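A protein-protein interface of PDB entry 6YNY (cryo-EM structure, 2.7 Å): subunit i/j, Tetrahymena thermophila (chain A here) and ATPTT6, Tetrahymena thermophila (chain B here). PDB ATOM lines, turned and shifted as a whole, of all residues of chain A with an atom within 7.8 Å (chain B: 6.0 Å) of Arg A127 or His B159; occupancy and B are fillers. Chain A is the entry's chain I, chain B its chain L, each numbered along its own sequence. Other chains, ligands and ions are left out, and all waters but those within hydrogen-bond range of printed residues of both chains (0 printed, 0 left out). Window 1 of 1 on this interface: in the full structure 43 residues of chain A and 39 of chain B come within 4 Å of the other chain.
O of Arg A127 is in hydrogen-bond range of NE2 of His B159, 2.7 Å away.
The side-chain carboxylate (OD1) of Asp B161 lies within hydrogen-bond range of the side-chain hydroxyl (OH) of Tyr A123 (3.1 Å).
NH1 of Arg A127 is in salt-bridge range of OD1 of Asp B161 (2.6 Å).
NE of Arg B163 lies within hydrogen-bond range of O of His B159 (3.0 Å).
OH of Tyr A123 is in hydrogen-bond range of NH1 of Arg A127 (2.9 Å).
Among the printed residues, pairs that only touch across the chains: Ala A128 with Leu B172 (3.5 Å), Leu A124 with Val B168 (3.7 Å) and Arg A127 with Leu B172 (3.9 Å).
Pro A122 touches none of the printed residues of chain B.
Of the printed residues of chain B, Leu A124 touches Val B168.
Of chain B, only His B159, Asp B161 and Leu B172 come within 4 Å of Arg A127.
Printed residues of chain B within 4 Å of Ala A128: Leu B172 (3.5 Å).
Of chain A, only Arg A127 (2.7 Å) comes within 4 Å of His B159.
Trp B160 touches none of the printed residues of chain A.
Of the printed residues of chain A, Asp B161 touches Tyr A123 (3.1 Å) and Arg A127 (2.6 Å).
Of the printed residues of chain A, Val B168 touches Leu A124 (3.7 Å).
Of the printed residues of chain A, Leu B172 touches Arg A127 and Ala A128.
Of the 9 printed residues of chain B, 4 touch a printed residue of chain A.
Printed residues of chain B that touch a printed residue of chain A: His B159, Asp B161, Val B168 and Leu B172.
Hydrophobic or aromatic side chains of chain B within 4 Å of the printed part of chain A: His B159, Val B168 and Leu B172.
Along chain B the printed residues that touch a printed residue of chain A span positions 159 to 172.
Of the 13 printed residues of chain A, 4 touch a printed residue of chain B.
Hydrophobic or aromatic side chains of chain A within 4 Å of the printed part of chain B: Tyr A123 and Leu A124.
Among the printed residues, Asp or Glu carboxylates within 4 Å of a Lys or Arg side-chain nitrogen of the other chain: Arg A127 with Asp B161.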
ATOM      1  N   PRO A 118       0.789 -25.120  -9.231  1.00  0.00           N
ATOM      2  CA  PRO A 118      -0.407 -25.591  -8.515  1.00  0.00           C
ATOM      3  C   PRO A 118      -0.556 -25.024  -7.118  1.00  0.00           C
ATOM      4  O   PRO A 118      -1.654 -25.100  -6.555  1.00  0.00           O
ATOM      5  CB  PRO A 118      -0.221 -27.112  -8.492  1.00  0.00           C
ATOM      6  CG  PRO A 118       0.660 -27.393  -9.629  1.00  0.00           C
ATOM      7  CD  PRO A 118       1.601 -26.249  -9.706  1.00  0.00           C
ATOM      8  N   PHE A 121      -2.428 -19.080  -7.037  1.00  0.00           N
ATOM      9  CA  PHE A 121      -3.831 -18.791  -7.314  1.00  0.00           C
ATOM     10  C   PHE A 121      -4.184 -18.848  -8.795  1.00  0.00           C
ATOM     11  O   PHE A 121      -5.269 -19.362  -9.120  1.00  0.00           O
ATOM     12  CB  PHE A 121      -4.174 -17.421  -6.719  1.00  0.00           C
ATOM     13  CG  PHE A 121      -5.543 -16.933  -7.056  1.00  0.00           C
ATOM     14  CD1 PHE A 121      -6.649 -17.424  -6.396  1.00  0.00           C
ATOM     15  CD2 PHE A 121      -5.724 -15.969  -8.024  1.00  0.00           C
ATOM     16  CE1 PHE A 121      -7.902 -16.972  -6.706  1.00  0.00           C
ATOM     17  CE2 PHE A 121      -6.977 -15.515  -8.333  1.00  0.00           C
ATOM     18  CZ  PHE A 121      -8.066 -16.017  -7.673  1.00  0.00           C
ATOM     19  N   PRO A 122      -3.363 -18.348  -9.720  1.00  0.00           N
ATOM     20  CA  PRO A 122      -3.746 -18.387 -11.141  1.00  0.00           C
ATOM     21  C   PRO A 122      -3.991 -19.780 -11.678  1.00  0.00           C
ATOM     22  O   PRO A 122      -4.706 -19.921 -12.677  1.00  0.00           O
ATOM     23  CB  PRO A 122      -2.553 -17.723 -11.838  1.00  0.00           C
ATOM     24  CG  PRO A 122      -1.913 -16.914 -10.802  1.00  0.00           C
ATOM     25  CD  PRO A 122      -2.082 -17.657  -9.531  1.00  0.00           C
ATOM     26  N   TYR A 123      -3.423 -20.815 -11.064  1.00  0.00           N
ATOM     27  CA  TYR A 123      -3.668 -22.172 -11.536  1.00  0.00           C
ATOM     28  C   TYR A 123      -5.116 -22.578 -11.305  1.00  0.00           C
ATOM     29  O   TYR A 123      -5.721 -23.249 -12.147  1.00  0.00           O
ATOM     30  CB  TYR A 123      -2.716 -23.139 -10.835  1.00  0.00           C
ATOM     31  CG  TYR A 123      -2.811 -24.570 -11.292  1.00  0.00           C
ATOM     32  CD1 TYR A 123      -2.227 -24.978 -12.477  1.00  0.00           C
ATOM     33  CD2 TYR A 123      -3.467 -25.519 -10.529  1.00  0.00           C
ATOM     34  CE1 TYR A 123      -2.303 -26.280 -12.894  1.00  0.00           C
ATOM     35  CE2 TYR A 123      -3.547 -26.826 -10.939  1.00  0.00           C
ATOM     36  CZ  TYR A 123      -2.963 -27.202 -12.122  1.00  0.00           C
ATOM     37  OH  TYR A 123      -3.043 -28.507 -12.535  1.00  0.00           O
ATOM     38  N   LEU A 124      -5.691 -22.172 -10.175  1.00  0.00           N
ATOM     39  CA  LEU A 124      -7.081 -22.501  -9.886  1.00  0.00           C
ATOM     40  C   LEU A 124      -8.015 -21.919 -10.935  1.00  0.00           C
ATOM     41  O   LEU A 124      -9.003 -22.555 -11.320  1.00  0.00           O
ATOM     42  CB  LEU A 124      -7.454 -21.990  -8.500  1.00  0.00           C
ATOM     43  CG  LEU A 124      -7.652 -23.010  -7.390  1.00  0.00           C
ATOM     44  CD1 LEU A 124      -6.515 -23.984  -7.334  1.00  0.00           C
ATOM     45  CD2 LEU A 124      -7.777 -22.273  -6.089  1.00  0.00           C
ATOM     46  N   LYS A 125      -7.723 -20.710 -11.407  1.00  0.00           N
ATOM     47  CA  LYS A 125      -8.577 -20.088 -12.411  1.00  0.00           C
ATOM     48  C   LYS A 125      -8.503 -20.825 -13.739  1.00  0.00           C
ATOM     49  O   LYS A 125      -9.514 -20.960 -14.438  1.00  0.00           O
ATOM     50  CB  LYS A 125      -8.190 -18.624 -12.590  1.00  0.00           C
ATOM     51  CG  LYS A 125      -8.411 -17.777 -11.362  1.00  0.00           C
ATOM     52  CD  LYS A 125      -8.348 -16.301 -11.679  1.00  0.00           C
ATOM     53  CE  LYS A 125      -6.993 -15.895 -12.201  1.00  0.00           C
ATOM     54  NZ  LYS A 125      -6.936 -14.448 -12.461  1.00  0.00           N
ATOM     55  N   LYS A 126      -7.318 -21.307 -14.110  1.00  0.00           N
ATOM     56  CA  LYS A 126      -7.188 -22.042 -15.360  1.00  0.00           C
ATOM     57  C   LYS A 126      -7.959 -23.353 -15.313  1.00  0.00           C
ATOM     58  O   LYS A 126      -8.573 -23.753 -16.307  1.00  0.00           O
ATOM     59  CB  LYS A 126      -5.716 -22.289 -15.670  1.00  0.00           C
ATOM     60  CG  LYS A 126      -5.012 -21.084 -16.256  1.00  0.00           C
ATOM     61  CD  LYS A 126      -3.610 -21.417 -16.716  1.00  0.00           C
ATOM     62  CE  LYS A 126      -2.569 -20.922 -15.748  1.00  0.00           C
ATOM     63  NZ  LYS A 126      -2.509 -19.438 -15.723  1.00  0.00           N
ATOM     64  N   ARG A 127      -7.943 -24.034 -14.171  1.00  0.00           N
ATOM     65  CA  ARG A 127      -8.677 -25.282 -14.043  1.00  0.00           C
ATOM     66  C   ARG A 127     -10.170 -25.057 -13.858  1.00  0.00           C
ATOM     67  O   ARG A 127     -10.956 -25.984 -14.078  1.00  0.00           O
ATOM     68  CB  ARG A 127      -8.128 -26.095 -12.875  1.00  0.00           C
ATOM     69  CG  ARG A 127      -6.627 -26.286 -12.902  1.00  0.00           C
ATOM     70  CD  ARG A 127      -6.134 -26.868 -14.208  1.00  0.00           C
ATOM     71  NE  ARG A 127      -6.865 -28.069 -14.591  1.00  0.00           N
ATOM     72  CZ  ARG A 127      -6.639 -29.271 -14.081  1.00  0.00           C
ATOM     73  NH1 ARG A 127      -5.705 -29.440 -13.162  1.00  0.00           N
ATOM     74  NH2 ARG A 127      -7.352 -30.306 -14.486  1.00  0.00           N
ATOM     75  N   ALA A 128     -10.575 -23.858 -13.455  1.00  0.00           N
ATOM     76  CA  ALA A 128     -11.980 -23.499 -13.360  1.00  0.00           C
ATOM     77  C   ALA A 128     -12.520 -22.908 -14.656  1.00  0.00           C
ATOM     78  O   ALA A 128     -13.595 -22.304 -14.647  1.00  0.00           O
ATOM     79  CB  ALA A 128     -12.195 -22.515 -12.213  1.00  0.00           C
ATOM     80  N   GLY A 129     -11.799 -23.064 -15.760  1.00  0.00           N
ATOM     81  CA  GLY A 129     -12.243 -22.534 -17.034  1.00  0.00           C
ATOM     82  C   GLY A 129     -11.901 -21.082 -17.258  1.00  0.00           C
ATOM     83  O   GLY A 129     -12.697 -20.348 -17.856  1.00  0.00           O
ATOM     84  N   ASP A 130     -10.734 -20.644 -16.799  1.00  0.00           N
ATOM     85  CA  ASP A 130     -10.326 -19.246 -16.884  1.00  0.00           C
ATOM     86  C   ASP A 130     -11.426 -18.342 -16.335  1.00  0.00           C
ATOM     87  O   ASP A 130     -11.945 -17.452 -17.011  1.00  0.00           O
ATOM     88  CB  ASP A 130      -9.960 -18.865 -18.316  1.00  0.00           C
ATOM     89  CG  ASP A 130      -9.402 -17.461 -18.415  1.00  0.00           C
ATOM     90  OD1 ASP A 130      -8.344 -17.201 -17.809  1.00  0.00           O
ATOM     91  OD2 ASP A 130     -10.019 -16.618 -19.098  1.00  0.00           O
ATOM     92  N   MET A 131     -11.775 -18.596 -15.083  1.00  0.00           N
ATOM     93  CA  MET A 131     -12.891 -17.941 -14.425  1.00  0.00           C
ATOM     94  C   MET A 131     -12.411 -17.277 -13.145  1.00  0.00           C
ATOM     95  O   MET A 131     -11.553 -17.812 -12.436  1.00  0.00           O
ATOM     96  CB  MET A 131     -13.991 -18.953 -14.121  1.00  0.00           C
ATOM     97  CG  MET A 131     -15.305 -18.354 -13.707  1.00  0.00           C
ATOM     98  SD  MET A 131     -16.613 -19.586 -13.667  1.00  0.00           S
ATOM     99  CE  MET A 131     -17.929 -18.616 -12.954  1.00  0.00           C
ATOM    100  N   LEU A 133     -12.171 -16.114  -9.429  1.00  0.00           N
ATOM    101  CA  LEU A 133     -12.460 -16.729  -8.147  1.00  0.00           C
ATOM    102  C   LEU A 133     -12.108 -15.771  -7.025  1.00  0.00           C
ATOM    103  O   LEU A 133     -11.317 -14.841  -7.215  1.00  0.00           O
ATOM    104  CB  LEU A 133     -11.662 -18.027  -7.970  1.00  0.00           C
ATOM    105  CG  LEU A 133     -11.833 -19.086  -9.051  1.00  0.00           C
ATOM    106  CD1 LEU A 133     -10.772 -20.139  -8.917  1.00  0.00           C
ATOM    107  CD2 LEU A 133     -13.202 -19.704  -8.953  1.00  0.00           C
ATOM    108  N   TRP B 157     -10.795 -38.843 -13.863  1.00  0.00           N
ATOM    109  CA  TRP B 157      -9.594 -38.054 -13.651  1.00  0.00           C
ATOM    110  C   TRP B 157      -9.743 -36.620 -14.134  1.00  0.00           C
ATOM    111  O   TRP B 157      -8.749 -35.892 -14.194  1.00  0.00           O
ATOM    112  CB  TRP B 157      -8.410 -38.724 -14.337  1.00  0.00           C
ATOM    113  CG  TRP B 157      -8.145 -40.097 -13.831  1.00  0.00           C
ATOM    114  CD1 TRP B 157      -7.505 -40.434 -12.681  1.00  0.00           C
ATOM    115  CD2 TRP B 157      -8.518 -41.327 -14.458  1.00  0.00           C
ATOM    116  NE1 TRP B 157      -7.455 -41.796 -12.549  1.00  0.00           N
ATOM    117  CE2 TRP B 157      -8.069 -42.368 -13.629  1.00  0.00           C
ATOM    118  CE3 TRP B 157      -9.186 -41.648 -15.641  1.00  0.00           C
ATOM    119  CZ2 TRP B 157      -8.266 -43.703 -13.943  1.00  0.00           C
ATOM    120  CZ3 TRP B 157      -9.379 -42.971 -15.947  1.00  0.00           C
ATOM    121  CH2 TRP B 157      -8.923 -43.984 -15.105  1.00  0.00           C
ATOM    122  N   ASN B 158     -10.953 -36.202 -14.488  1.00  0.00           N
ATOM    123  CA  ASN B 158     -11.198 -34.802 -14.787  1.00  0.00           C
ATOM    124  C   ASN B 158     -11.039 -33.972 -13.523  1.00  0.00           C
ATOM    125  O   ASN B 158     -11.680 -34.245 -12.504  1.00  0.00           O
ATOM    126  CB  ASN B 158     -12.602 -34.611 -15.357  1.00  0.00           C
ATOM    127  CG  ASN B 158     -12.860 -35.443 -16.591  1.00  0.00           C
ATOM    128  OD1 ASN B 158     -13.921 -36.046 -16.731  1.00  0.00           O
ATOM    129  ND2 ASN B 158     -11.898 -35.479 -17.494  1.00  0.00           N
ATOM    130  N   HIS B 159     -10.181 -32.957 -13.584  1.00  0.00           N
ATOM    131  CA  HIS B 159      -9.973 -32.048 -12.461  1.00  0.00           C
ATOM    132  C   HIS B 159      -9.533 -32.797 -11.206  1.00  0.00           C
ATOM    133  O   HIS B 159      -9.925 -32.452 -10.090  1.00  0.00           O
ATOM    134  CB  HIS B 159     -11.238 -31.241 -12.172  1.00  0.00           C
ATOM    135  CG  HIS B 159     -11.580 -30.232 -13.221  1.00  0.00           C
ATOM    136  ND1 HIS B 159     -12.647 -30.385 -14.077  1.00  0.00           N
ATOM    137  CD2 HIS B 159     -11.013 -29.045 -13.535  1.00  0.00           C
ATOM    138  CE1 HIS B 159     -12.717 -29.341 -14.881  1.00  0.00           C
ATOM    139  NE2 HIS B 159     -11.735 -28.513 -14.574  1.00  0.00           N
ATOM    140  N   TRP B 160      -8.704 -33.826 -11.379  1.00  0.00           N
ATOM    141  CA  TRP B 160      -8.372 -34.686 -10.249  1.00  0.00           C
ATOM    142  C   TRP B 160      -7.509 -33.975  -9.217  1.00  0.00           C
ATOM    143  O   TRP B 160      -7.579 -34.302  -8.029  1.00  0.00           O
ATOM    144  CB  TRP B 160      -7.677 -35.954 -10.738  1.00  0.00           C
ATOM    145  CG  TRP B 160      -6.292 -35.760 -11.254  1.00  0.00           C
ATOM    146  CD1 TRP B 160      -5.918 -35.646 -12.554  1.00  0.00           C
ATOM    147  CD2 TRP B 160      -5.090 -35.675 -10.482  1.00  0.00           C
ATOM    148  NE1 TRP B 160      -4.563 -35.489 -12.644  1.00  0.00           N
ATOM    149  CE2 TRP B 160      -4.030 -35.502 -11.385  1.00  0.00           C
ATOM    150  CE3 TRP B 160      -4.808 -35.723  -9.115  1.00  0.00           C
ATOM    151  CZ2 TRP B 160      -2.712 -35.376 -10.968  1.00  0.00           C
ATOM    152  CZ3 TRP B 160      -3.503 -35.596  -8.707  1.00  0.00           C
ATOM    153  CH2 TRP B 160      -2.470 -35.425  -9.629  1.00  0.00           C
ATOM    154  N   ASP B 161      -6.697 -33.012  -9.638  1.00  0.00           N
ATOM    155  CA  ASP B 161      -5.785 -32.320  -8.740  1.00  0.00           C
ATOM    156  C   ASP B 161      -6.376 -31.049  -8.146  1.00  0.00           C
ATOM    157  O   ASP B 161      -5.654 -30.299  -7.484  1.00  0.00           O
ATOM    158  CB  ASP B 161      -4.481 -31.997  -9.467  1.00  0.00           C
ATOM    159  CG  ASP B 161      -4.704 -31.303 -10.787  1.00  0.00           C
ATOM    160  OD1 ASP B 161      -4.993 -30.091 -10.785  1.00  0.00           O
ATOM    161  OD2 ASP B 161      -4.592 -31.974 -11.834  1.00  0.00           O
ATOM    162  N   VAL B 162      -7.663 -30.791  -8.362  1.00  0.00           N
ATOM    163  CA  VAL B 162      -8.323 -29.626  -7.785  1.00  0.00           C
ATOM    164  C   VAL B 162      -9.624 -30.025  -7.103  1.00  0.00           C
ATOM    165  O   VAL B 162     -10.429 -29.163  -6.739  1.00  0.00           O
ATOM    166  CB  VAL B 162      -8.577 -28.547  -8.851  1.00  0.00           C
ATOM    167  CG1 VAL B 162      -7.284 -27.883  -9.240  1.00  0.00           C
ATOM    168  CG2 VAL B 162      -9.241 -29.144 -10.060  1.00  0.00           C
ATOM    169  N   ARG B 163      -9.844 -31.327  -6.920  1.00  0.00           N
ATOM    170  CA  ARG B 163     -11.051 -31.762  -6.231  1.00  0.00           C
ATOM    171  C   ARG B 163     -11.089 -31.272  -4.793  1.00  0.00           C
ATOM    172  O   ARG B 163     -12.173 -31.183  -4.208  1.00  0.00           O
ATOM    173  CB  ARG B 163     -11.164 -33.286  -6.254  1.00  0.00           C
ATOM    174  CG  ARG B 163     -11.164 -33.908  -7.630  1.00  0.00           C
ATOM    175  CD  ARG B 163     -12.271 -33.357  -8.492  1.00  0.00           C
ATOM    176  NE  ARG B 163     -12.383 -34.054  -9.766  1.00  0.00           N
ATOM    177  CZ  ARG B 163     -13.137 -35.127  -9.974  1.00  0.00           C
ATOM    178  NH1 ARG B 163     -13.168 -35.686 -11.170  1.00  0.00           N
ATOM    179  NH2 ARG B 163     -13.862 -35.642  -8.998  1.00  0.00           N
ATOM    180  N   VAL B 168     -13.667 -23.970  -6.748  1.00  0.00           N
ATOM    181  CA  VAL B 168     -13.545 -24.450  -8.118  1.00  0.00           C
ATOM    182  C   VAL B 168     -14.758 -25.281  -8.506  1.00  0.00           C
ATOM    183  O   VAL B 168     -15.199 -25.246  -9.659  1.00  0.00           O
ATOM    184  CB  VAL B 168     -12.242 -25.249  -8.286  1.00  0.00           C
ATOM    185  CG1 VAL B 168     -12.118 -25.765  -9.696  1.00  0.00           C
ATOM    186  CG2 VAL B 168     -11.049 -24.395  -7.942  1.00  0.00           C
ATOM    187  N   LEU B 172     -17.563 -24.190 -11.571  1.00  0.00           N
ATOM    188  CA  LEU B 172     -17.737 -25.056 -12.729  1.00  0.00           C
ATOM    189  C   LEU B 172     -19.145 -25.626 -12.815  1.00  0.00           C
ATOM    190  O   LEU B 172     -19.706 -25.734 -13.911  1.00  0.00           O
ATOM    191  CB  LEU B 172     -16.726 -26.198 -12.679  1.00  0.00           C
ATOM    192  CG  LEU B 172     -15.263 -25.815 -12.838  1.00  0.00           C
ATOM    193  CD1 LEU B 172     -14.390 -26.947 -12.383  1.00  0.00           C
ATOM    194  CD2 LEU B 172     -14.974 -25.479 -14.271  1.00  0.00           C
